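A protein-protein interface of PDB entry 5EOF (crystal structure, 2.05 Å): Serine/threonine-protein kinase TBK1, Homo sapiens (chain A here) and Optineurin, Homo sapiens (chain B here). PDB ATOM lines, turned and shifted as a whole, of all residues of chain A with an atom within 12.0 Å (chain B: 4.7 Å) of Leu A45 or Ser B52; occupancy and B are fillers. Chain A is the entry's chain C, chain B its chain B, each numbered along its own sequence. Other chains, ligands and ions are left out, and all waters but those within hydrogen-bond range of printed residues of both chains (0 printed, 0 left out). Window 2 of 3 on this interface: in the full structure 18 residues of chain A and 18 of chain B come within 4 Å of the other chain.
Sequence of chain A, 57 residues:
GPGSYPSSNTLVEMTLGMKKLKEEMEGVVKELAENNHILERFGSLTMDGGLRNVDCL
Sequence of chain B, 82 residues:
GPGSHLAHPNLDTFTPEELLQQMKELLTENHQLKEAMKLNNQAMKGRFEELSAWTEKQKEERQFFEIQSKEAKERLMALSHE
CG2 of Ile A38 touches CB of Phe B48, at 3.9 Å. Phe B48 touches Arg A41 (CE1 to O, 3.5 Å). Phe A42 touches Phe B48. Leu B51 touches Phe A42 (CD1 to CE2, 3.3 Å). Phe B48 touches Leu A45 (CE1 to CD2, 3.7 Å). Leu B51 touches Leu A45 (CB to CD1, 3.6 Å). Ser B52 touches Leu A45. Thr B55 touches Leu A45 (OG1 to O, 3.9 Å). Lys B59 touches Leu A45 (NZ to O, 3.5 Å). O of Met A47 touches NZ of Lys B59, 3.8 Å away.
The side-chain hydroxyl (OG) of Ser B52 lies within hydrogen-bond range of the backbone carbonyl oxygen (O) of Phe B48 (2.9 Å). The side-chain hydroxyl (OG1) of Thr B55 is in hydrogen-bond range of the backbone carbonyl oxygen (O) of Leu B51. The side-chain hydroxyl (OG1) of Thr B55 is in hydrogen-bond range of the backbone carbonyl oxygen (O) of Ser B52, at 3.0 Å. O of Arg A41 lies within hydrogen-bond range of OG of Ser A44 (2.9 Å).
Of the 10 printed residues of chain B, 5 touch a printed residue of chain A. Hydrophobic or aromatic side chains of chain A that line the printed part of chain B: Ile A38, Phe A42 and Leu A45. Among the printed residues, 10 pairs touch across the chains.
Of the printed residues of chain B, Ile A38 touches Phe B48. Printed residues of chain B within 4 Å of Phe A42: Phe B48 and Leu B51. Ser A44 touches none of the printed residues of chain B. Of the printed residues of chain A, Leu B51 touches Phe A42 (3.3 Å) and Leu A45 (3.6 Å). Of the printed residues of chain A, Ser B52 touches Leu A45. Thr B55 touches one residue of chain A. No residue of chain A comes within 4 Å of Glu B56. The nearest printed residue of chain B that does not touch Leu A45 is Glu B56 (6.2 Å). The nearest printed residue of chain A that does not touch Ser B52 is Arg A41 (6.8 Å). The nearest printed residue of chain A that does not touch Leu B51 is Thr A46 (7.6 Å).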
ATOM      1  N   ASN A  35      11.972   2.140  20.164  1.00  0.00           N
ATOM      2  CA  ASN A  35      12.080   0.703  19.905  1.00  0.00           C
ATOM      3  C   ASN A  35      10.927  -0.049  20.595  1.00  0.00           C
ATOM      4  O   ASN A  35      10.219  -0.836  19.961  1.00  0.00           O
ATOM      5  CB  ASN A  35      13.430   0.203  20.442  1.00  0.00           C
ATOM      6  CG  ASN A  35      14.082  -0.861  19.563  1.00  0.00           C
ATOM      7  OD1 ASN A  35      14.125  -2.055  19.920  1.00  0.00           O
ATOM      8  ND2 ASN A  35      14.632  -0.429  18.424  1.00  0.00           N
ATOM      9  N   HIS A  37       8.057   1.047  21.646  1.00  0.00           N
ATOM     10  CA  HIS A  37       6.785   1.415  21.039  1.00  0.00           C
ATOM     11  C   HIS A  37       6.559   0.625  19.751  1.00  0.00           C
ATOM     12  O   HIS A  37       5.502   0.010  19.562  1.00  0.00           O
ATOM     13  CB  HIS A  37       6.765   2.915  20.752  1.00  0.00           C
ATOM     14  CG  HIS A  37       5.589   3.358  19.949  1.00  0.00           C
ATOM     15  ND1 HIS A  37       4.289   3.131  20.348  1.00  0.00           N
ATOM     16  CD2 HIS A  37       5.513   4.017  18.768  1.00  0.00           C
ATOM     17  CE1 HIS A  37       3.461   3.627  19.443  1.00  0.00           C
ATOM     18  NE2 HIS A  37       4.178   4.175  18.476  1.00  0.00           N
ATOM     19  N   ILE A  38       7.555   0.618  18.868  1.00  0.00           N
ATOM     20  CA  ILE A  38       7.405  -0.115  17.606  1.00  0.00           C
ATOM     21  C   ILE A  38       7.188  -1.615  17.830  1.00  0.00           C
ATOM     22  O   ILE A  38       6.341  -2.242  17.165  1.00  0.00           O
ATOM     23  CB  ILE A  38       8.593   0.146  16.670  1.00  0.00           C
ATOM     24  CG1 ILE A  38       8.780   1.658  16.532  1.00  0.00           C
ATOM     25  CG2 ILE A  38       8.353  -0.493  15.308  1.00  0.00           C
ATOM     26  CD1 ILE A  38       9.884   2.069  15.599  1.00  0.00           C
ATOM     27  N   LEU A  39       7.931  -2.184  18.776  1.00  0.00           N
ATOM     28  CA  LEU A  39       7.777  -3.596  19.126  1.00  0.00           C
ATOM     29  C   LEU A  39       6.358  -3.906  19.598  1.00  0.00           C
ATOM     30  O   LEU A  39       5.773  -4.921  19.221  1.00  0.00           O
ATOM     31  CB  LEU A  39       8.786  -3.988  20.206  1.00  0.00           C
ATOM     32  CG  LEU A  39       8.642  -5.357  20.869  1.00  0.00           C
ATOM     33  CD1 LEU A  39       8.700  -6.497  19.822  1.00  0.00           C
ATOM     34  CD2 LEU A  39       9.734  -5.545  21.920  1.00  0.00           C
ATOM     35  N   GLU A  40       5.810  -3.030  20.429  1.00  0.00           N
ATOM     36  CA  GLU A  40       4.431  -3.169  20.880  1.00  0.00           C
ATOM     37  C   GLU A  40       3.489  -3.245  19.678  1.00  0.00           C
ATOM     38  O   GLU A  40       2.618  -4.119  19.609  1.00  0.00           O
ATOM     39  CB  GLU A  40       4.056  -1.996  21.791  1.00  0.00           C
ATOM     40  CG  GLU A  40       2.868  -2.246  22.719  1.00  0.00           C
ATOM     41  CD  GLU A  40       2.559  -1.049  23.627  1.00  0.00           C
ATOM     42  OE1 GLU A  40       3.512  -0.432  24.165  1.00  0.00           O
ATOM     43  OE2 GLU A  40       1.359  -0.724  23.801  1.00  0.00           O
ATOM     44  N   ARG A  41       3.687  -2.359  18.708  1.00  0.00           N
ATOM     45  CA  ARG A  41       2.859  -2.386  17.488  1.00  0.00           C
ATOM     46  C   ARG A  41       3.024  -3.651  16.625  1.00  0.00           C
ATOM     47  O   ARG A  41       2.119  -4.012  15.848  1.00  0.00           O
ATOM     48  CB  ARG A  41       3.115  -1.131  16.648  1.00  0.00           C
ATOM     49  CG  ARG A  41       2.719   0.173  17.331  1.00  0.00           C
ATOM     50  CD  ARG A  41       1.222   0.284  17.501  1.00  0.00           C
ATOM     51  NE  ARG A  41       0.879   1.607  17.998  1.00  0.00           N
ATOM     52  CZ  ARG A  41       0.596   2.649  17.226  1.00  0.00           C
ATOM     53  NH1 ARG A  41       0.583   2.527  15.904  1.00  0.00           N
ATOM     54  NH2 ARG A  41       0.317   3.814  17.779  1.00  0.00           N
ATOM     55  N   PHE A  42       4.169  -4.322  16.749  1.00  0.00           N
ATOM     56  CA  PHE A  42       4.416  -5.550  15.983  1.00  0.00           C
ATOM     57  C   PHE A  42       3.392  -6.605  16.375  1.00  0.00           C
ATOM     58  O   PHE A  42       2.964  -7.399  15.551  1.00  0.00           O
ATOM     59  CB  PHE A  42       5.819  -6.112  16.264  1.00  0.00           C
ATOM     60  CG  PHE A  42       6.870  -5.720  15.255  1.00  0.00           C
ATOM     61  CD1 PHE A  42       7.459  -4.472  15.285  1.00  0.00           C
ATOM     62  CD2 PHE A  42       7.310  -6.626  14.310  1.00  0.00           C
ATOM     63  CE1 PHE A  42       8.443  -4.125  14.372  1.00  0.00           C
ATOM     64  CE2 PHE A  42       8.302  -6.274  13.404  1.00  0.00           C
ATOM     65  CZ  PHE A  42       8.857  -5.023  13.434  1.00  0.00           C
ATOM     66  N   GLY A  43       3.015  -6.621  17.649  1.00  0.00           N
ATOM     67  CA  GLY A  43       2.062  -7.594  18.144  1.00  0.00           C
ATOM     68  C   GLY A  43       0.639  -7.407  17.638  1.00  0.00           C
ATOM     69  O   GLY A  43      -0.223  -8.233  17.923  1.00  0.00           O
ATOM     70  N   SER A  44       0.387  -6.343  16.877  1.00  0.00           N
ATOM     71  CA  SER A  44      -0.961  -6.055  16.383  1.00  0.00           C
ATOM     72  C   SER A  44      -1.126  -6.294  14.884  1.00  0.00           C
ATOM     73  O   SER A  44      -2.227  -6.148  14.351  1.00  0.00           O
ATOM     74  CB  SER A  44      -1.361  -4.611  16.703  1.00  0.00           C
ATOM     75  OG  SER A  44      -0.726  -3.691  15.821  1.00  0.00           O
ATOM     76  N   LEU A  45      -0.044  -6.652  14.194  1.00  0.00           N
ATOM     77  CA  LEU A  45      -0.126  -6.849  12.734  1.00  0.00           C
ATOM     78  C   LEU A  45      -1.084  -7.957  12.270  1.00  0.00           C
ATOM     79  O   LEU A  45      -1.748  -7.818  11.243  1.00  0.00           O
ATOM     80  CB  LEU A  45       1.259  -7.057  12.115  1.00  0.00           C
ATOM     81  CG  LEU A  45       2.187  -5.841  12.193  1.00  0.00           C
ATOM     82  CD1 LEU A  45       3.545  -6.179  11.617  1.00  0.00           C
ATOM     83  CD2 LEU A  45       1.588  -4.679  11.448  1.00  0.00           C
ATOM     84  N   THR A  46      -1.158  -9.051  13.015  1.00  0.00           N
ATOM     85  CA  THR A  46      -2.022 -10.159  12.623  1.00  0.00           C
ATOM     86  C   THR A  46      -3.353 -10.176  13.370  1.00  0.00           C
ATOM     87  O   THR A  46      -3.871 -11.242  13.707  1.00  0.00           O
ATOM     88  CB  THR A  46      -1.330 -11.494  12.839  1.00  0.00           C
ATOM     89  OG1 THR A  46      -1.076 -11.677  14.235  1.00  0.00           O
ATOM     90  CG2 THR A  46      -0.035 -11.520  12.076  1.00  0.00           C
ATOM     91  N   MET A  47      -3.907  -8.995  13.617  1.00  0.00           N
ATOM     92  CA  MET A  47      -5.131  -8.875  14.400  1.00  0.00           C
ATOM     93  C   MET A  47      -6.138  -7.964  13.705  1.00  0.00           C
ATOM     94  O   MET A  47      -5.746  -6.911  13.195  1.00  0.00           O
ATOM     95  CB  MET A  47      -4.809  -8.310  15.785  1.00  0.00           C
ATOM     96  CG  MET A  47      -3.887  -9.177  16.629  1.00  0.00           C
ATOM     97  SD  MET A  47      -4.713 -10.601  17.358  1.00  0.00           S
ATOM     98  CE  MET A  47      -5.951  -9.763  18.343  1.00  0.00           C
ATOM     99  N   ASP A  48      -7.400  -8.418  13.677  1.00  0.00           N
ATOM    100  CA  ASP A  48      -8.636  -7.690  13.283  1.00  0.00           C
ATOM    101  C   ASP A  48      -9.507  -8.504  12.331  1.00  0.00           C
ATOM    102  O   ASP A  48     -10.338  -9.299  12.767  1.00  0.00           O
ATOM    103  CB  ASP A  48      -8.412  -6.282  12.709  1.00  0.00           C
ATOM    104  CG  ASP A  48      -8.038  -5.267  13.777  1.00  0.00           C
ATOM    105  OD1 ASP A  48      -8.451  -5.440  14.945  1.00  0.00           O
ATOM    106  OD2 ASP A  48      -7.321  -4.300  13.444  1.00  0.00           O
ATOM    107  N   PHE B  48       8.704  -2.598  10.204  1.00  0.00           N
ATOM    108  CA  PHE B  48       7.310  -2.496  10.603  1.00  0.00           C
ATOM    109  C   PHE B  48       6.479  -2.088   9.391  1.00  0.00           C
ATOM    110  O   PHE B  48       5.411  -2.648   9.166  1.00  0.00           O
ATOM    111  CB  PHE B  48       7.062  -1.515  11.754  1.00  0.00           C
ATOM    112  CG  PHE B  48       5.595  -1.386  12.120  1.00  0.00           C
ATOM    113  CD1 PHE B  48       4.999  -2.290  12.993  1.00  0.00           C
ATOM    114  CD2 PHE B  48       4.799  -0.398  11.548  1.00  0.00           C
ATOM    115  CE1 PHE B  48       3.638  -2.199  13.309  1.00  0.00           C
ATOM    116  CE2 PHE B  48       3.445  -0.304  11.859  1.00  0.00           C
ATOM    117  CZ  PHE B  48       2.863  -1.205  12.744  1.00  0.00           C
ATOM    118  N   GLU B  49       6.973  -1.127   8.614  1.00  0.00           N
ATOM    119  CA  GLU B  49       6.242  -0.678   7.436  1.00  0.00           C
ATOM    120  C   GLU B  49       6.097  -1.810   6.411  1.00  0.00           C
ATOM    121  O   GLU B  49       5.025  -1.996   5.838  1.00  0.00           O
ATOM    122  CB  GLU B  49       6.923   0.533   6.803  1.00  0.00           C
ATOM    123  CG  GLU B  49       6.780   1.821   7.595  1.00  0.00           C
ATOM    124  CD  GLU B  49       7.761   2.897   7.140  1.00  0.00           C
ATOM    125  OE1 GLU B  49       8.554   2.630   6.207  1.00  0.00           O
ATOM    126  OE2 GLU B  49       7.737   4.007   7.714  1.00  0.00           O
ATOM    127  N   GLU B  50       7.169  -2.574   6.203  1.00  0.00           N
ATOM    128  CA  GLU B  50       7.155  -3.664   5.226  1.00  0.00           C
ATOM    129  C   GLU B  50       6.237  -4.783   5.668  1.00  0.00           C
ATOM    130  O   GLU B  50       5.539  -5.374   4.845  1.00  0.00           O
ATOM    131  CB  GLU B  50       8.557  -4.242   5.020  1.00  0.00           C
ATOM    132  CG  GLU B  50       9.527  -3.334   4.311  1.00  0.00           C
ATOM    133  CD  GLU B  50      10.980  -3.757   4.557  1.00  0.00           C
ATOM    134  OE1 GLU B  50      11.206  -4.869   5.108  1.00  0.00           O
ATOM    135  OE2 GLU B  50      11.892  -2.976   4.207  1.00  0.00           O
ATOM    136  N   LEU B  51       6.238  -5.089   6.961  1.00  0.00           N
ATOM    137  CA  LEU B  51       5.400  -6.169   7.462  1.00  0.00           C
ATOM    138  C   LEU B  51       3.925  -5.797   7.429  1.00  0.00           C
ATOM    139  O   LEU B  51       3.074  -6.650   7.174  1.00  0.00           O
ATOM    140  CB  LEU B  51       5.796  -6.580   8.869  1.00  0.00           C
ATOM    141  CG  LEU B  51       7.150  -7.271   9.010  1.00  0.00           C
ATOM    142  CD1 LEU B  51       7.408  -7.417  10.469  1.00  0.00           C
ATOM    143  CD2 LEU B  51       7.156  -8.632   8.340  1.00  0.00           C
ATOM    144  N   SER B  52       3.631  -4.523   7.682  1.00  0.00           N
ATOM    145  CA  SER B  52       2.262  -4.016   7.607  1.00  0.00           C
ATOM    146  C   SER B  52       1.709  -4.207   6.205  1.00  0.00           C
ATOM    147  O   SER B  52       0.628  -4.790   6.017  1.00  0.00           O
ATOM    148  CB  SER B  52       2.204  -2.527   7.970  1.00  0.00           C
ATOM    149  OG  SER B  52       2.544  -2.321   9.323  1.00  0.00           O
ATOM    150  N   ALA B  53       2.454  -3.710   5.224  1.00  0.00           N
ATOM    151  CA  ALA B  53       2.087  -3.838   3.824  1.00  0.00           C
ATOM    152  C   ALA B  53       1.876  -5.309   3.443  1.00  0.00           C
ATOM    153  O   ALA B  53       0.903  -5.668   2.777  1.00  0.00           O
ATOM    154  CB  ALA B  53       3.156  -3.215   2.954  1.00  0.00           C
ATOM    155  N   TRP B  54       2.795  -6.152   3.893  1.00  0.00           N
ATOM    156  CA  TRP B  54       2.797  -7.578   3.585  1.00  0.00           C
ATOM    157  C   TRP B  54       1.622  -8.316   4.210  1.00  0.00           C
ATOM    158  O   TRP B  54       0.937  -9.098   3.525  1.00  0.00           O
ATOM    159  CB  TRP B  54       4.126  -8.165   4.043  1.00  0.00           C
ATOM    160  CG  TRP B  54       4.322  -9.634   3.886  1.00  0.00           C
ATOM    161  CD1 TRP B  54       4.564 -10.322   2.726  1.00  0.00           C
ATOM    162  CD2 TRP B  54       4.391 -10.591   4.944  1.00  0.00           C
ATOM    163  NE1 TRP B  54       4.749 -11.658   3.004  1.00  0.00           N
ATOM    164  CE2 TRP B  54       4.655 -11.847   4.359  1.00  0.00           C
ATOM    165  CE3 TRP B  54       4.258 -10.509   6.337  1.00  0.00           C
ATOM    166  CZ2 TRP B  54       4.780 -13.015   5.120  1.00  0.00           C
ATOM    167  CZ3 TRP B  54       4.379 -11.666   7.092  1.00  0.00           C
ATOM    168  CH2 TRP B  54       4.639 -12.906   6.479  1.00  0.00           C
ATOM    169  N   THR B  55       1.366  -8.079   5.495  1.00  0.00           N
ATOM    170  CA  THR B  55       0.201  -8.708   6.127  1.00  0.00           C
ATOM    171  C   THR B  55      -1.104  -8.248   5.465  1.00  0.00           C
ATOM    172  O   THR B  55      -2.044  -9.039   5.281  1.00  0.00           O
ATOM    173  CB  THR B  55       0.133  -8.454   7.643  1.00  0.00           C
ATOM    174  OG1 THR B  55       0.142  -7.046   7.878  1.00  0.00           O
ATOM    175  CG2 THR B  55       1.324  -9.097   8.358  1.00  0.00           C
ATOM    176  N   GLU B  56      -1.162  -6.968   5.112  1.00  0.00           N
ATOM    177  CA  GLU B  56      -2.353  -6.429   4.462  1.00  0.00           C
ATOM    178  C   GLU B  56      -2.591  -7.102   3.115  1.00  0.00           C
ATOM    179  O   GLU B  56      -3.724  -7.443   2.770  1.00  0.00           O
ATOM    180  CB  GLU B  56      -2.233  -4.912   4.272  1.00  0.00           C
ATOM    181  CG  GLU B  56      -3.563  -4.215   3.996  1.00  0.00           C
ATOM    182  CD  GLU B  56      -4.572  -4.423   5.120  1.00  0.00           C
ATOM    183  OE1 GLU B  56      -4.181  -4.308   6.306  1.00  0.00           O
ATOM    184  OE2 GLU B  56      -5.752  -4.711   4.820  1.00  0.00           O
ATOM    185  N   LYS B  59      -4.157 -10.553   3.609  1.00  0.00           N
ATOM    186  CA  LYS B  59      -5.570 -10.474   4.000  1.00  0.00           C
ATOM    187  C   LYS B  59      -6.433 -10.220   2.766  1.00  0.00           C
ATOM    188  O   LYS B  59      -7.431 -10.917   2.537  1.00  0.00           O
ATOM    189  CB  LYS B  59      -5.789  -9.358   5.026  1.00  0.00           C
ATOM    190  CG  LYS B  59      -5.076  -9.576   6.364  1.00  0.00           C
ATOM    191  CD  LYS B  59      -5.186  -8.337   7.253  1.00  0.00           C
ATOM    192  CE  LYS B  59      -4.595  -8.569   8.635  1.00  0.00           C
ATOM    193  NZ  LYS B  59      -4.760  -7.368   9.502  1.00  0.00           N
